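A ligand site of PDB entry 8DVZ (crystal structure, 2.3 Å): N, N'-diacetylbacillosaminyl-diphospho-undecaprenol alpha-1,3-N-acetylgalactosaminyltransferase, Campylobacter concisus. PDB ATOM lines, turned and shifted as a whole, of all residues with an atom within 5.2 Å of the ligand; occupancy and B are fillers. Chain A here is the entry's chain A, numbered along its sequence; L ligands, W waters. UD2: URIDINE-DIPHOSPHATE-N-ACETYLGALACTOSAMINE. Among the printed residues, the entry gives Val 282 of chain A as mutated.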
ATOM      1  N   PHE A  16      14.468  18.496 -11.500  1.00  0.00           N
ATOM      2  CA  PHE A  16      13.392  18.897 -10.596  1.00  0.00           C
ATOM      3  C   PHE A  16      13.887  19.331  -9.225  1.00  0.00           C
ATOM      4  O   PHE A  16      13.287  20.210  -8.604  1.00  0.00           O
ATOM      5  CB  PHE A  16      12.386  17.751 -10.398  1.00  0.00           C
ATOM      6  CG  PHE A  16      11.475  17.509 -11.571  1.00  0.00           C
ATOM      7  CD1 PHE A  16      10.544  18.458 -11.947  1.00  0.00           C
ATOM      8  CD2 PHE A  16      11.551  16.329 -12.285  1.00  0.00           C
ATOM      9  CE1 PHE A  16       9.701  18.232 -13.033  1.00  0.00           C
ATOM     10  CE2 PHE A  16      10.722  16.086 -13.366  1.00  0.00           C
ATOM     11  CZ  PHE A  16       9.792  17.044 -13.732  1.00  0.00           C
ATOM     12  N   PHE A  17      14.962  18.708  -8.716  1.00  0.00           N
ATOM     13  CA  PHE A  17      15.376  18.890  -7.331  1.00  0.00           C
ATOM     14  C   PHE A  17      16.677  19.682  -7.208  1.00  0.00           C
ATOM     15  O   PHE A  17      16.712  20.703  -6.520  1.00  0.00           O
ATOM     16  CB  PHE A  17      15.522  17.525  -6.629  1.00  0.00           C
ATOM     17  CG  PHE A  17      14.332  16.628  -6.778  1.00  0.00           C
ATOM     18  CD1 PHE A  17      13.055  17.147  -6.891  1.00  0.00           C
ATOM     19  CD2 PHE A  17      14.484  15.248  -6.791  1.00  0.00           C
ATOM     20  CE1 PHE A  17      11.951  16.323  -7.032  1.00  0.00           C
ATOM     21  CE2 PHE A  17      13.386  14.411  -6.930  1.00  0.00           C
ATOM     22  CZ  PHE A  17      12.119  14.948  -7.050  1.00  0.00           C
ATOM     23  N   ARG A  18      17.743  19.231  -7.873  1.00  0.00           N
ATOM     24  CA  ARG A  18      19.038  19.893  -7.731  1.00  0.00           C
ATOM     25  C   ARG A  18      19.086  21.235  -8.431  1.00  0.00           C
ATOM     26  O   ARG A  18      19.972  22.048  -8.132  1.00  0.00           O
ATOM     27  CB  ARG A  18      20.169  19.014  -8.301  1.00  0.00           C
ATOM     28  CG  ARG A  18      20.193  17.573  -7.809  1.00  0.00           C
ATOM     29  CD  ARG A  18      20.672  17.483  -6.360  1.00  0.00           C
ATOM     30  NE  ARG A  18      19.611  17.774  -5.409  1.00  0.00           N
ATOM     31  CZ  ARG A  18      18.726  16.895  -4.980  1.00  0.00           C
ATOM     32  NH1 ARG A  18      18.736  15.637  -5.400  1.00  0.00           N
ATOM     33  NH2 ARG A  18      17.802  17.271  -4.088  1.00  0.00           N
ATOM     34  N   GLU A 113      17.204  11.859   0.465  1.00  0.00           N
ATOM     35  CA  GLU A 113      15.865  12.407   0.235  1.00  0.00           C
ATOM     36  C   GLU A 113      14.883  11.230   0.188  1.00  0.00           C
ATOM     37  O   GLU A 113      14.302  10.905  -0.852  1.00  0.00           O
ATOM     38  CB  GLU A 113      15.819  13.247  -1.045  1.00  0.00           C
ATOM     39  CG  GLU A 113      16.324  12.567  -2.311  1.00  0.00           C
ATOM     40  CD  GLU A 113      16.737  13.576  -3.374  1.00  0.00           C
ATOM     41  OE1 GLU A 113      16.352  14.763  -3.260  1.00  0.00           O
ATOM     42  OE2 GLU A 113      17.453  13.195  -4.336  1.00  0.00           O
ATOM     43  N   GLY A 114      14.694  10.587   1.337  1.00  0.00           N
ATOM     44  CA  GLY A 114      13.840   9.426   1.439  1.00  0.00           C
ATOM     45  C   GLY A 114      14.645   8.145   1.519  1.00  0.00           C
ATOM     46  O   GLY A 114      15.682   8.019   0.855  1.00  0.00           O
ATOM     47  N   LEU A 115      14.183   7.190   2.322  1.00  0.00           N
ATOM     48  CA  LEU A 115      14.915   5.942   2.526  1.00  0.00           C
ATOM     49  C   LEU A 115      14.501   4.863   1.530  1.00  0.00           C
ATOM     50  O   LEU A 115      15.250   3.900   1.339  1.00  0.00           O
ATOM     51  CB  LEU A 115      14.715   5.439   3.956  1.00  0.00           C
ATOM     52  CG  LEU A 115      15.282   6.360   5.035  1.00  0.00           C
ATOM     53  CD1 LEU A 115      15.061   5.752   6.426  1.00  0.00           C
ATOM     54  CD2 LEU A 115      16.763   6.650   4.817  1.00  0.00           C
ATOM     55  N   GLY A 116      13.342   4.993   0.897  1.00  0.00           N
ATOM     56  CA  GLY A 116      12.994   4.131  -0.213  1.00  0.00           C
ATOM     57  C   GLY A 116      12.428   2.794   0.196  1.00  0.00           C
ATOM     58  O   GLY A 116      12.122   2.520   1.359  1.00  0.00           O
ATOM     59  N   VAL A 150      16.731  16.020   3.707  1.00  0.00           N
ATOM     60  CA  VAL A 150      15.597  16.889   3.389  1.00  0.00           C
ATOM     61  C   VAL A 150      14.461  16.769   4.399  1.00  0.00           C
ATOM     62  O   VAL A 150      13.530  17.586   4.361  1.00  0.00           O
ATOM     63  CB  VAL A 150      15.067  16.605   1.976  1.00  0.00           C
ATOM     64  CG1 VAL A 150      16.204  16.694   0.956  1.00  0.00           C
ATOM     65  CG2 VAL A 150      14.382  15.250   1.902  1.00  0.00           C
ATOM     66  N   VAL A 175      13.544  20.213  -0.739  1.00  0.00           N
ATOM     67  CA  VAL A 175      14.409  20.678  -1.819  1.00  0.00           C
ATOM     68  C   VAL A 175      13.869  21.984  -2.380  1.00  0.00           C
ATOM     69  O   VAL A 175      14.346  22.487  -3.411  1.00  0.00           O
ATOM     70  CB  VAL A 175      14.534  19.618  -2.929  1.00  0.00           C
ATOM     71  CG1 VAL A 175      15.095  18.313  -2.361  1.00  0.00           C
ATOM     72  CG2 VAL A 175      13.178  19.376  -3.597  1.00  0.00           C
ATOM     73  N   PHE A 182       4.966  28.664  -9.110  1.00  0.00           N
ATOM     74  CA  PHE A 182       3.808  27.972  -8.541  1.00  0.00           C
ATOM     75  C   PHE A 182       2.966  28.978  -7.747  1.00  0.00           C
ATOM     76  O   PHE A 182       2.808  28.899  -6.534  1.00  0.00           O
ATOM     77  CB  PHE A 182       4.262  26.819  -7.661  1.00  0.00           C
ATOM     78  CG  PHE A 182       4.616  25.580  -8.429  1.00  0.00           C
ATOM     79  CD1 PHE A 182       5.898  25.376  -8.905  1.00  0.00           C
ATOM     80  CD2 PHE A 182       3.657  24.602  -8.658  1.00  0.00           C
ATOM     81  CE1 PHE A 182       6.224  24.235  -9.598  1.00  0.00           C
ATOM     82  CE2 PHE A 182       3.980  23.452  -9.353  1.00  0.00           C
ATOM     83  CZ  PHE A 182       5.260  23.271  -9.829  1.00  0.00           C
ATOM     84  N   ILE A 201      -0.485  13.216  -8.103  1.00  0.00           N
ATOM     85  CA  ILE A 201       0.649  13.334  -9.008  1.00  0.00           C
ATOM     86  C   ILE A 201       1.726  12.379  -8.530  1.00  0.00           C
ATOM     87  O   ILE A 201       2.272  12.568  -7.428  1.00  0.00           O
ATOM     88  CB  ILE A 201       1.194  14.763  -9.066  1.00  0.00           C
ATOM     89  CG1 ILE A 201       0.135  15.755  -9.549  1.00  0.00           C
ATOM     90  CG2 ILE A 201       2.429  14.820  -9.979  1.00  0.00           C
ATOM     91  CD1 ILE A 201       0.448  17.182  -9.157  1.00  0.00           C
ATOM     92  N   ALA A 202       2.068  11.389  -9.345  1.00  0.00           N
ATOM     93  CA  ALA A 202       3.147  10.491  -8.971  1.00  0.00           C
ATOM     94  C   ALA A 202       3.498   9.478 -10.046  1.00  0.00           C
ATOM     95  O   ALA A 202       2.631   9.033 -10.803  1.00  0.00           O
ATOM     96  CB  ALA A 202       2.785   9.746  -7.680  1.00  0.00           C
ATOM     97  N   ARG A 203       4.780   9.112 -10.121  1.00  0.00           N
ATOM     98  CA  ARG A 203       5.156   7.842 -10.724  1.00  0.00           C
ATOM     99  C   ARG A 203       4.266   6.751 -10.149  1.00  0.00           C
ATOM    100  O   ARG A 203       4.028   6.694  -8.942  1.00  0.00           O
ATOM    101  CB  ARG A 203       6.629   7.537 -10.439  1.00  0.00           C
ATOM    102  CG  ARG A 203       7.316   6.668 -11.475  1.00  0.00           C
ATOM    103  CD  ARG A 203       8.728   6.322 -11.030  1.00  0.00           C
ATOM    104  NE  ARG A 203       9.197   5.080 -11.633  1.00  0.00           N
ATOM    105  CZ  ARG A 203       9.681   4.978 -12.863  1.00  0.00           C
ATOM    106  NH1 ARG A 203       9.789   6.027 -13.649  1.00  0.00           N
ATOM    107  NH2 ARG A 203      10.059   3.783 -13.307  1.00  0.00           N
ATOM    108  N   LYS A 208       3.746   4.200  -3.890  1.00  0.00           N
ATOM    109  CA  LYS A 208       3.204   5.546  -3.850  1.00  0.00           C
ATOM    110  C   LYS A 208       1.745   5.589  -3.434  1.00  0.00           C
ATOM    111  O   LYS A 208       1.198   6.678  -3.237  1.00  0.00           O
ATOM    112  CB  LYS A 208       3.378   6.224  -5.215  1.00  0.00           C
ATOM    113  CG  LYS A 208       4.779   6.745  -5.470  1.00  0.00           C
ATOM    114  CD  LYS A 208       5.015   8.032  -4.693  1.00  0.00           C
ATOM    115  CE  LYS A 208       6.369   8.643  -4.996  1.00  0.00           C
ATOM    116  NZ  LYS A 208       6.342  10.104  -4.739  1.00  0.00           N
ATOM    117  N   VAL A 231      -1.974  11.898 -12.395  1.00  0.00           N
ATOM    118  CA  VAL A 231      -0.942  12.391 -13.292  1.00  0.00           C
ATOM    119  C   VAL A 231       0.336  11.620 -12.999  1.00  0.00           C
ATOM    120  O   VAL A 231       0.746  11.519 -11.837  1.00  0.00           O
ATOM    121  CB  VAL A 231      -0.721  13.906 -13.121  1.00  0.00           C
ATOM    122  CG1 VAL A 231       0.515  14.356 -13.896  1.00  0.00           C
ATOM    123  CG2 VAL A 231      -1.957  14.672 -13.579  1.00  0.00           C
ATOM    124  N   GLY A 232       0.955  11.083 -14.047  1.00  0.00           N
ATOM    125  CA  GLY A 232       2.215  10.380 -13.887  1.00  0.00           C
ATOM    126  C   GLY A 232       2.287   9.108 -14.708  1.00  0.00           C
ATOM    127  O   GLY A 232       1.259   8.626 -15.203  1.00  0.00           O
ATOM    128  N   GLY A 256      -1.552  10.535 -17.773  1.00  0.00           N
ATOM    129  CA  GLY A 256      -0.171  10.273 -18.110  1.00  0.00           C
ATOM    130  C   GLY A 256       0.750  11.380 -17.598  1.00  0.00           C
ATOM    131  O   GLY A 256       0.388  12.186 -16.727  1.00  0.00           O
ATOM    132  N   ALA A 257       1.961  11.398 -18.150  1.00  0.00           N
ATOM    133  CA  ALA A 257       2.938  12.416 -17.788  1.00  0.00           C
ATOM    134  C   ALA A 257       2.449  13.792 -18.205  1.00  0.00           C
ATOM    135  O   ALA A 257       1.728  13.948 -19.187  1.00  0.00           O
ATOM    136  CB  ALA A 257       4.283  12.114 -18.443  1.00  0.00           C
ATOM    137  N   ARG A 258       2.860  14.816 -17.443  1.00  0.00           N
ATOM    138  CA  ARG A 258       2.461  16.173 -17.745  1.00  0.00           C
ATOM    139  C   ARG A 258       3.570  17.143 -17.328  1.00  0.00           C
ATOM    140  O   ARG A 258       4.392  16.843 -16.460  1.00  0.00           O
ATOM    141  CB  ARG A 258       1.157  16.560 -17.034  1.00  0.00           C
ATOM    142  CG  ARG A 258      -0.022  15.656 -17.326  1.00  0.00           C
ATOM    143  CD  ARG A 258      -0.742  16.048 -18.614  1.00  0.00           C
ATOM    144  NE  ARG A 258      -1.253  17.405 -18.584  1.00  0.00           N
ATOM    145  CZ  ARG A 258      -2.440  17.784 -19.047  1.00  0.00           C
ATOM    146  NH1 ARG A 258      -3.271  16.906 -19.592  1.00  0.00           N
ATOM    147  NH2 ARG A 258      -2.804  19.053 -18.957  1.00  0.00           N
ATOM    148  N   ASN A 259       3.557  18.316 -17.964  1.00  0.00           N
ATOM    149  CA  ASN A 259       4.473  19.396 -17.644  1.00  0.00           C
ATOM    150  C   ASN A 259       3.774  20.626 -17.086  1.00  0.00           C
ATOM    151  O   ASN A 259       4.458  21.538 -16.602  1.00  0.00           O
ATOM    152  CB  ASN A 259       5.280  19.818 -18.880  1.00  0.00           C
ATOM    153  CG  ASN A 259       5.458  18.688 -19.866  1.00  0.00           C
ATOM    154  OD1 ASN A 259       6.061  17.658 -19.537  1.00  0.00           O
ATOM    155  ND2 ASN A 259       4.944  18.857 -21.073  1.00  0.00           N
ATOM    156  N   ILE A 261       2.041  21.229 -14.377  1.00  0.00           N
ATOM    157  CA  ILE A 261       1.639  20.922 -13.004  1.00  0.00           C
ATOM    158  C   ILE A 261       1.004  22.136 -12.352  1.00  0.00           C
ATOM    159  O   ILE A 261      -0.100  22.008 -11.785  1.00  0.00           O
ATOM    160  CB  ILE A 261       2.827  20.389 -12.204  1.00  0.00           C
ATOM    161  CG1 ILE A 261       3.389  19.104 -12.838  1.00  0.00           C
ATOM    162  CG2 ILE A 261       2.428  20.125 -10.755  1.00  0.00           C
ATOM    163  CD1 ILE A 261       2.352  18.031 -13.094  1.00  0.00           C
ATOM    164  N   SER A 275       1.216   7.899  -0.032  1.00  0.00           N
ATOM    165  CA  SER A 275       2.464   7.157  -0.193  1.00  0.00           C
ATOM    166  C   SER A 275       2.767   6.311   1.027  1.00  0.00           C
ATOM    167  O   SER A 275       2.315   6.578   2.141  1.00  0.00           O
ATOM    168  CB  SER A 275       3.618   8.133  -0.446  1.00  0.00           C
ATOM    169  OG  SER A 275       4.841   7.427  -0.552  1.00  0.00           O
ATOM    170  N   LYS A 277       6.016   5.804   1.953  1.00  0.00           N
ATOM    171  CA  LYS A 277       7.211   6.401   2.546  1.00  0.00           C
ATOM    172  C   LYS A 277       7.729   7.482   1.603  1.00  0.00           C
ATOM    173  O   LYS A 277       7.726   7.299   0.389  1.00  0.00           O
ATOM    174  CB  LYS A 277       8.288   5.347   2.792  1.00  0.00           C
ATOM    175  CG  LYS A 277       9.373   5.775   3.760  1.00  0.00           C
ATOM    176  CD  LYS A 277      10.213   4.589   4.232  1.00  0.00           C
ATOM    177  CE  LYS A 277       9.851   4.183   5.661  1.00  0.00           C
ATOM    178  NZ  LYS A 277      10.578   4.997   6.667  1.00  0.00           N
ATOM    179  N   GLU A 278       8.188   8.587   2.192  1.00  0.00           N
ATOM    180  CA  GLU A 278       8.633   9.739   1.425  1.00  0.00           C
ATOM    181  C   GLU A 278       9.846  10.361   2.098  1.00  0.00           C
ATOM    182  O   GLU A 278      10.239   9.994   3.201  1.00  0.00           O
ATOM    183  CB  GLU A 278       7.511  10.783   1.301  1.00  0.00           C
ATOM    184  CG  GLU A 278       6.306  10.328   0.483  1.00  0.00           C
ATOM    185  CD  GLU A 278       6.633  10.180  -0.990  1.00  0.00           C
ATOM    186  OE1 GLU A 278       7.424  10.987  -1.503  1.00  0.00           O
ATOM    187  OE2 GLU A 278       6.091   9.256  -1.638  1.00  0.00           O
ATOM    188  N   GLY A 279      10.460  11.319   1.388  1.00  0.00           N
ATOM    189  CA  GLY A 279      11.508  12.140   1.964  1.00  0.00           C
ATOM    190  C   GLY A 279      10.944  13.457   2.440  1.00  0.00           C
ATOM    191  O   GLY A 279      10.759  13.672   3.644  1.00  0.00           O
ATOM    192  N   PHE A 280      10.664  14.356   1.492  1.00  0.00           N
ATOM    193  CA  PHE A 280       9.809  15.516   1.743  1.00  0.00           C
ATOM    194  C   PHE A 280       9.037  15.734   0.449  1.00  0.00           C
ATOM    195  O   PHE A 280       9.513  16.427  -0.467  1.00  0.00           O
ATOM    196  CB  PHE A 280      10.602  16.764   2.138  1.00  0.00           C
ATOM    197  CG  PHE A 280       9.751  17.825   2.791  1.00  0.00           C
ATOM    198  CD1 PHE A 280       8.776  18.480   2.062  1.00  0.00           C
ATOM    199  CD2 PHE A 280       9.928  18.151   4.118  1.00  0.00           C
ATOM    200  CE1 PHE A 280       7.990  19.459   2.653  1.00  0.00           C
ATOM    201  CE2 PHE A 280       9.147  19.126   4.721  1.00  0.00           C
ATOM    202  CZ  PHE A 280       8.179  19.782   3.973  1.00  0.00           C
ATOM    203  N   PRO A 281       7.838  15.159   0.339  1.00  0.00           N
ATOM    204  CA  PRO A 281       7.212  15.032  -0.990  1.00  0.00           C
ATOM    205  C   PRO A 281       7.056  16.379  -1.685  1.00  0.00           C
ATOM    206  O   PRO A 281       6.519  17.328  -1.127  1.00  0.00           O
ATOM    207  CB  PRO A 281       5.850  14.389  -0.669  1.00  0.00           C
ATOM    208  CG  PRO A 281       5.571  14.795   0.757  1.00  0.00           C
ATOM    209  CD  PRO A 281       6.919  14.791   1.433  1.00  0.00           C
ATOM    210  N   VAL A 282       7.545  16.439  -2.924  1.00  0.00           N
ATOM    211  CA  VAL A 282       7.579  17.703  -3.650  1.00  0.00           C
ATOM    212  C   VAL A 282       6.205  18.049  -4.208  1.00  0.00           C
ATOM    213  O   VAL A 282       5.850  19.230  -4.295  1.00  0.00           O
ATOM    214  CB  VAL A 282       8.645  17.624  -4.747  1.00  0.00           C
ATOM    215  CG1 VAL A 282       8.519  18.779  -5.717  1.00  0.00           C
ATOM    216  CG2 VAL A 282      10.044  17.604  -4.106  1.00  0.00           C
ATOM    217  N   THR A 283       5.405  17.052  -4.595  1.00  0.00           N
ATOM    218  CA  THR A 283       4.056  17.362  -5.038  1.00  0.00           C
ATOM    219  C   THR A 283       3.243  18.009  -3.919  1.00  0.00           C
ATOM    220  O   THR A 283       2.352  18.819  -4.187  1.00  0.00           O
ATOM    221  CB  THR A 283       3.348  16.095  -5.542  1.00  0.00           C
ATOM    222  OG1 THR A 283       3.309  15.114  -4.501  1.00  0.00           O
ATOM    223  CG2 THR A 283       4.068  15.529  -6.756  1.00  0.00           C
ATOM    224  N   GLU A 286       4.299  21.583  -3.949  1.00  0.00           N
ATOM    225  CA  GLU A 286       3.690  22.259  -5.093  1.00  0.00           C
ATOM    226  C   GLU A 286       2.225  22.554  -4.838  1.00  0.00           C
ATOM    227  O   GLU A 286       1.754  23.665  -5.112  1.00  0.00           O
ATOM    228  CB  GLU A 286       3.891  21.394  -6.346  1.00  0.00           C
ATOM    229  CG  GLU A 286       5.327  21.482  -6.864  1.00  0.00           C
ATOM    230  CD  GLU A 286       5.685  20.404  -7.874  1.00  0.00           C
ATOM    231  OE1 GLU A 286       4.845  19.514  -8.137  1.00  0.00           O
ATOM    232  OE2 GLU A 286       6.813  20.453  -8.411  1.00  0.00           O
HETATM  233  C1' UD2 L   1      12.012  11.627  -3.702  1.00  0.00           C
HETATM  234  C2' UD2 L   1      11.045  11.504  -2.519  1.00  0.00           C
HETATM  235  C3' UD2 L   1      10.281  12.785  -2.311  1.00  0.00           C
HETATM  236  C4' UD2 L   1      11.212  13.998  -2.302  1.00  0.00           C
HETATM  237  C5' UD2 L   1      12.158  14.026  -3.514  1.00  0.00           C
HETATM  238  C6' UD2 L   1      13.084  15.226  -3.475  1.00  0.00           C
HETATM  239  C7' UD2 L   1      10.216   9.143  -2.189  1.00  0.00           C
HETATM  240  C8' UD2 L   1      11.337   8.770  -1.252  1.00  0.00           C
HETATM  241  N2' UD2 L   1      10.138  10.404  -2.721  1.00  0.00           N
HETATM  242  O1' UD2 L   1      11.626  11.766  -5.056  1.00  0.00           O
HETATM  243  O3' UD2 L   1       9.597  12.730  -1.096  1.00  0.00           O
HETATM  244  O4' UD2 L   1      11.952  13.870  -1.103  1.00  0.00           O
HETATM  245  O5' UD2 L   1      12.848  12.770  -3.536  1.00  0.00           O
HETATM  246  O6' UD2 L   1      13.535  15.614  -2.204  1.00  0.00           O
HETATM  247  O7' UD2 L   1       9.353   8.315  -2.439  1.00  0.00           O
HETATM  248  N1  UD2 L   1       6.195  15.600 -11.928  1.00  0.00           N
HETATM  249  C2  UD2 L   1       5.977  16.146 -13.183  1.00  0.00           C
HETATM  250  N3  UD2 L   1       5.121  15.445 -14.000  1.00  0.00           N
HETATM  251  C4  UD2 L   1       4.453  14.269 -13.688  1.00  0.00           C
HETATM  252  C5  UD2 L   1       4.740  13.783 -12.357  1.00  0.00           C
HETATM  253  C6  UD2 L   1       5.569  14.442 -11.549  1.00  0.00           C
HETATM  254  O2  UD2 L   1       6.463  17.151 -13.619  1.00  0.00           O
HETATM  255  O4  UD2 L   1       3.726  13.769 -14.524  1.00  0.00           O
HETATM  256  C1B UD2 L   1       7.118  16.294 -11.014  1.00  0.00           C
HETATM  257  C2B UD2 L   1       6.394  17.217 -10.033  1.00  0.00           C
HETATM  258  O2' UD2 L   1       6.098  18.468 -10.575  1.00  0.00           O
HETATM  259  C3B UD2 L   1       7.409  17.335  -8.889  1.00  0.00           C
HETATM  260  C4B UD2 L   1       8.092  15.976  -8.924  1.00  0.00           C
HETATM  261  O4B UD2 L   1       7.871  15.414 -10.223  1.00  0.00           O
HETATM  262  O3B UD2 L   1       8.393  18.326  -9.158  1.00  0.00           O
HETATM  263  C5B UD2 L   1       7.520  15.064  -7.872  1.00  0.00           C
HETATM  264  O5B UD2 L   1       8.519  14.262  -7.336  1.00  0.00           O
HETATM  265  PA  UD2 L   1       8.101  13.266  -6.106  1.00  0.00           P
HETATM  266  O1A UD2 L   1       7.589  14.063  -4.969  1.00  0.00           O
HETATM  267  O2A UD2 L   1       7.340  12.122  -6.733  1.00  0.00           O
HETATM  268  O3A UD2 L   1       9.599  12.849  -5.633  1.00  0.00           O
HETATM  269  PB  UD2 L   1      10.269  11.403  -5.947  1.00  0.00           P
HETATM  270  O1B UD2 L   1       9.449  10.285  -5.380  1.00  0.00           O
HETATM  271  O2B UD2 L   1      10.664  11.417  -7.376  1.00  0.00           O
HETATM  272  O   HOH W   1       7.004  11.838 -10.656  1.00  0.00           O
HETATM  273  O   HOH W   2       4.370  11.881  -5.729  1.00  0.00           O
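N of Val 282 sits at hydrogen-bond distance from O1A of the ligand (3.1 Å).
O3' of the ligand lies within hydrogen-bond range of N of Gly 279 (3.0 Å).
The backbone NH (N) of Arg 258 is in hydrogen-bond range of an oxygen (O4) of the ligand, at 3.2 Å.
The side-chain carboxylate of Glu 286 sits at hydrogen-bond distance from an oxygen (O3B) of the ligand (2.8 Å).
The side-chain amino group (NZ) of Lys 208 lies within salt-bridge range of an oxygen (O2A) of the ligand, at 3.0 Å.
The backbone carbonyl oxygen (O) of Arg 258 lies within hydrogen-bond range of a nitrogen (N3) of the ligand, 2.9 Å away.
The side-chain carboxylate (OE1) of Glu 278 lies within hydrogen-bond range of an oxygen (O3') of the ligand (2.8 Å).
An oxygen (O4') of the ligand sits at hydrogen-bond distance from the backbone NH (N) of Phe 280.
OE1 of Glu 113 sits at hydrogen-bond distance from O6' of the ligand (3.1 Å).
O of Gly 256 lies within hydrogen-bond range of N of Gly 232 (3.0 Å).
The side-chain carboxylate (OE2) of Glu 278 is in salt-bridge range of the side-chain amino group (NZ) of Lys 208.
The backbone carbonyl oxygen (O) of Lys 277 sits at hydrogen-bond distance from the side-chain hydroxyl (OG) of Ser 275, at 3.0 Å.
The backbone carbonyl oxygen (O) of Val 231 sits at hydrogen-bond distance from the backbone NH (N) of Ala 202 (2.8 Å).
The side-chain carboxylate (OE2) of Glu 113 is in salt-bridge range of the guanidinium group (NH1) of Arg 18, 3.0 Å away.
N of Ser 275 sits close to O of Lys 208, at 3.4 Å.
OE2 of Glu 278 lies within hydrogen-bond range of OG of Ser 275.
O of Lys 277 sits close to O7' of the ligand, 3.4 Å away.
An oxygen (O3') of the ligand lies close to the backbone nitrogen of Pro 281, 3.3 Å away.
Phe 16 touches the ligand (CZ to O2, 3.3 Å).
CE2 of Phe 17 touches C6' of the ligand (3.6 Å).
Gly 114 touches the ligand.
Val 175 touches the ligand (CG1 to O6', 3.1 Å).
CG2 of Ile 201 touches C5 of the ligand (3.5 Å).
Val 231 touches the ligand (CG1 to O4, 3.3 Å).
CA of Gly 232 touches O4 of the ligand (3.8 Å).
Ala 257 touches the ligand.
Ile 261 touches the ligand (CG1 to O2', 3.6 Å).
Thr 283 touches the ligand.
Hydrophobic or aromatic side chains that line the ligand: Phe 16, Phe 17, Val 175, Ile 201, Val 231, Ile 261 and Val 282.
The nearest printed residue that does not touch the ligand is Val 150 (4.1 Å).
Water W2 lies within hydrogen-bond range of O of Ile 201 (2.8 Å), NZ of Lys 208 (2.8 Å) and O2A of the ligand (3.1 Å).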
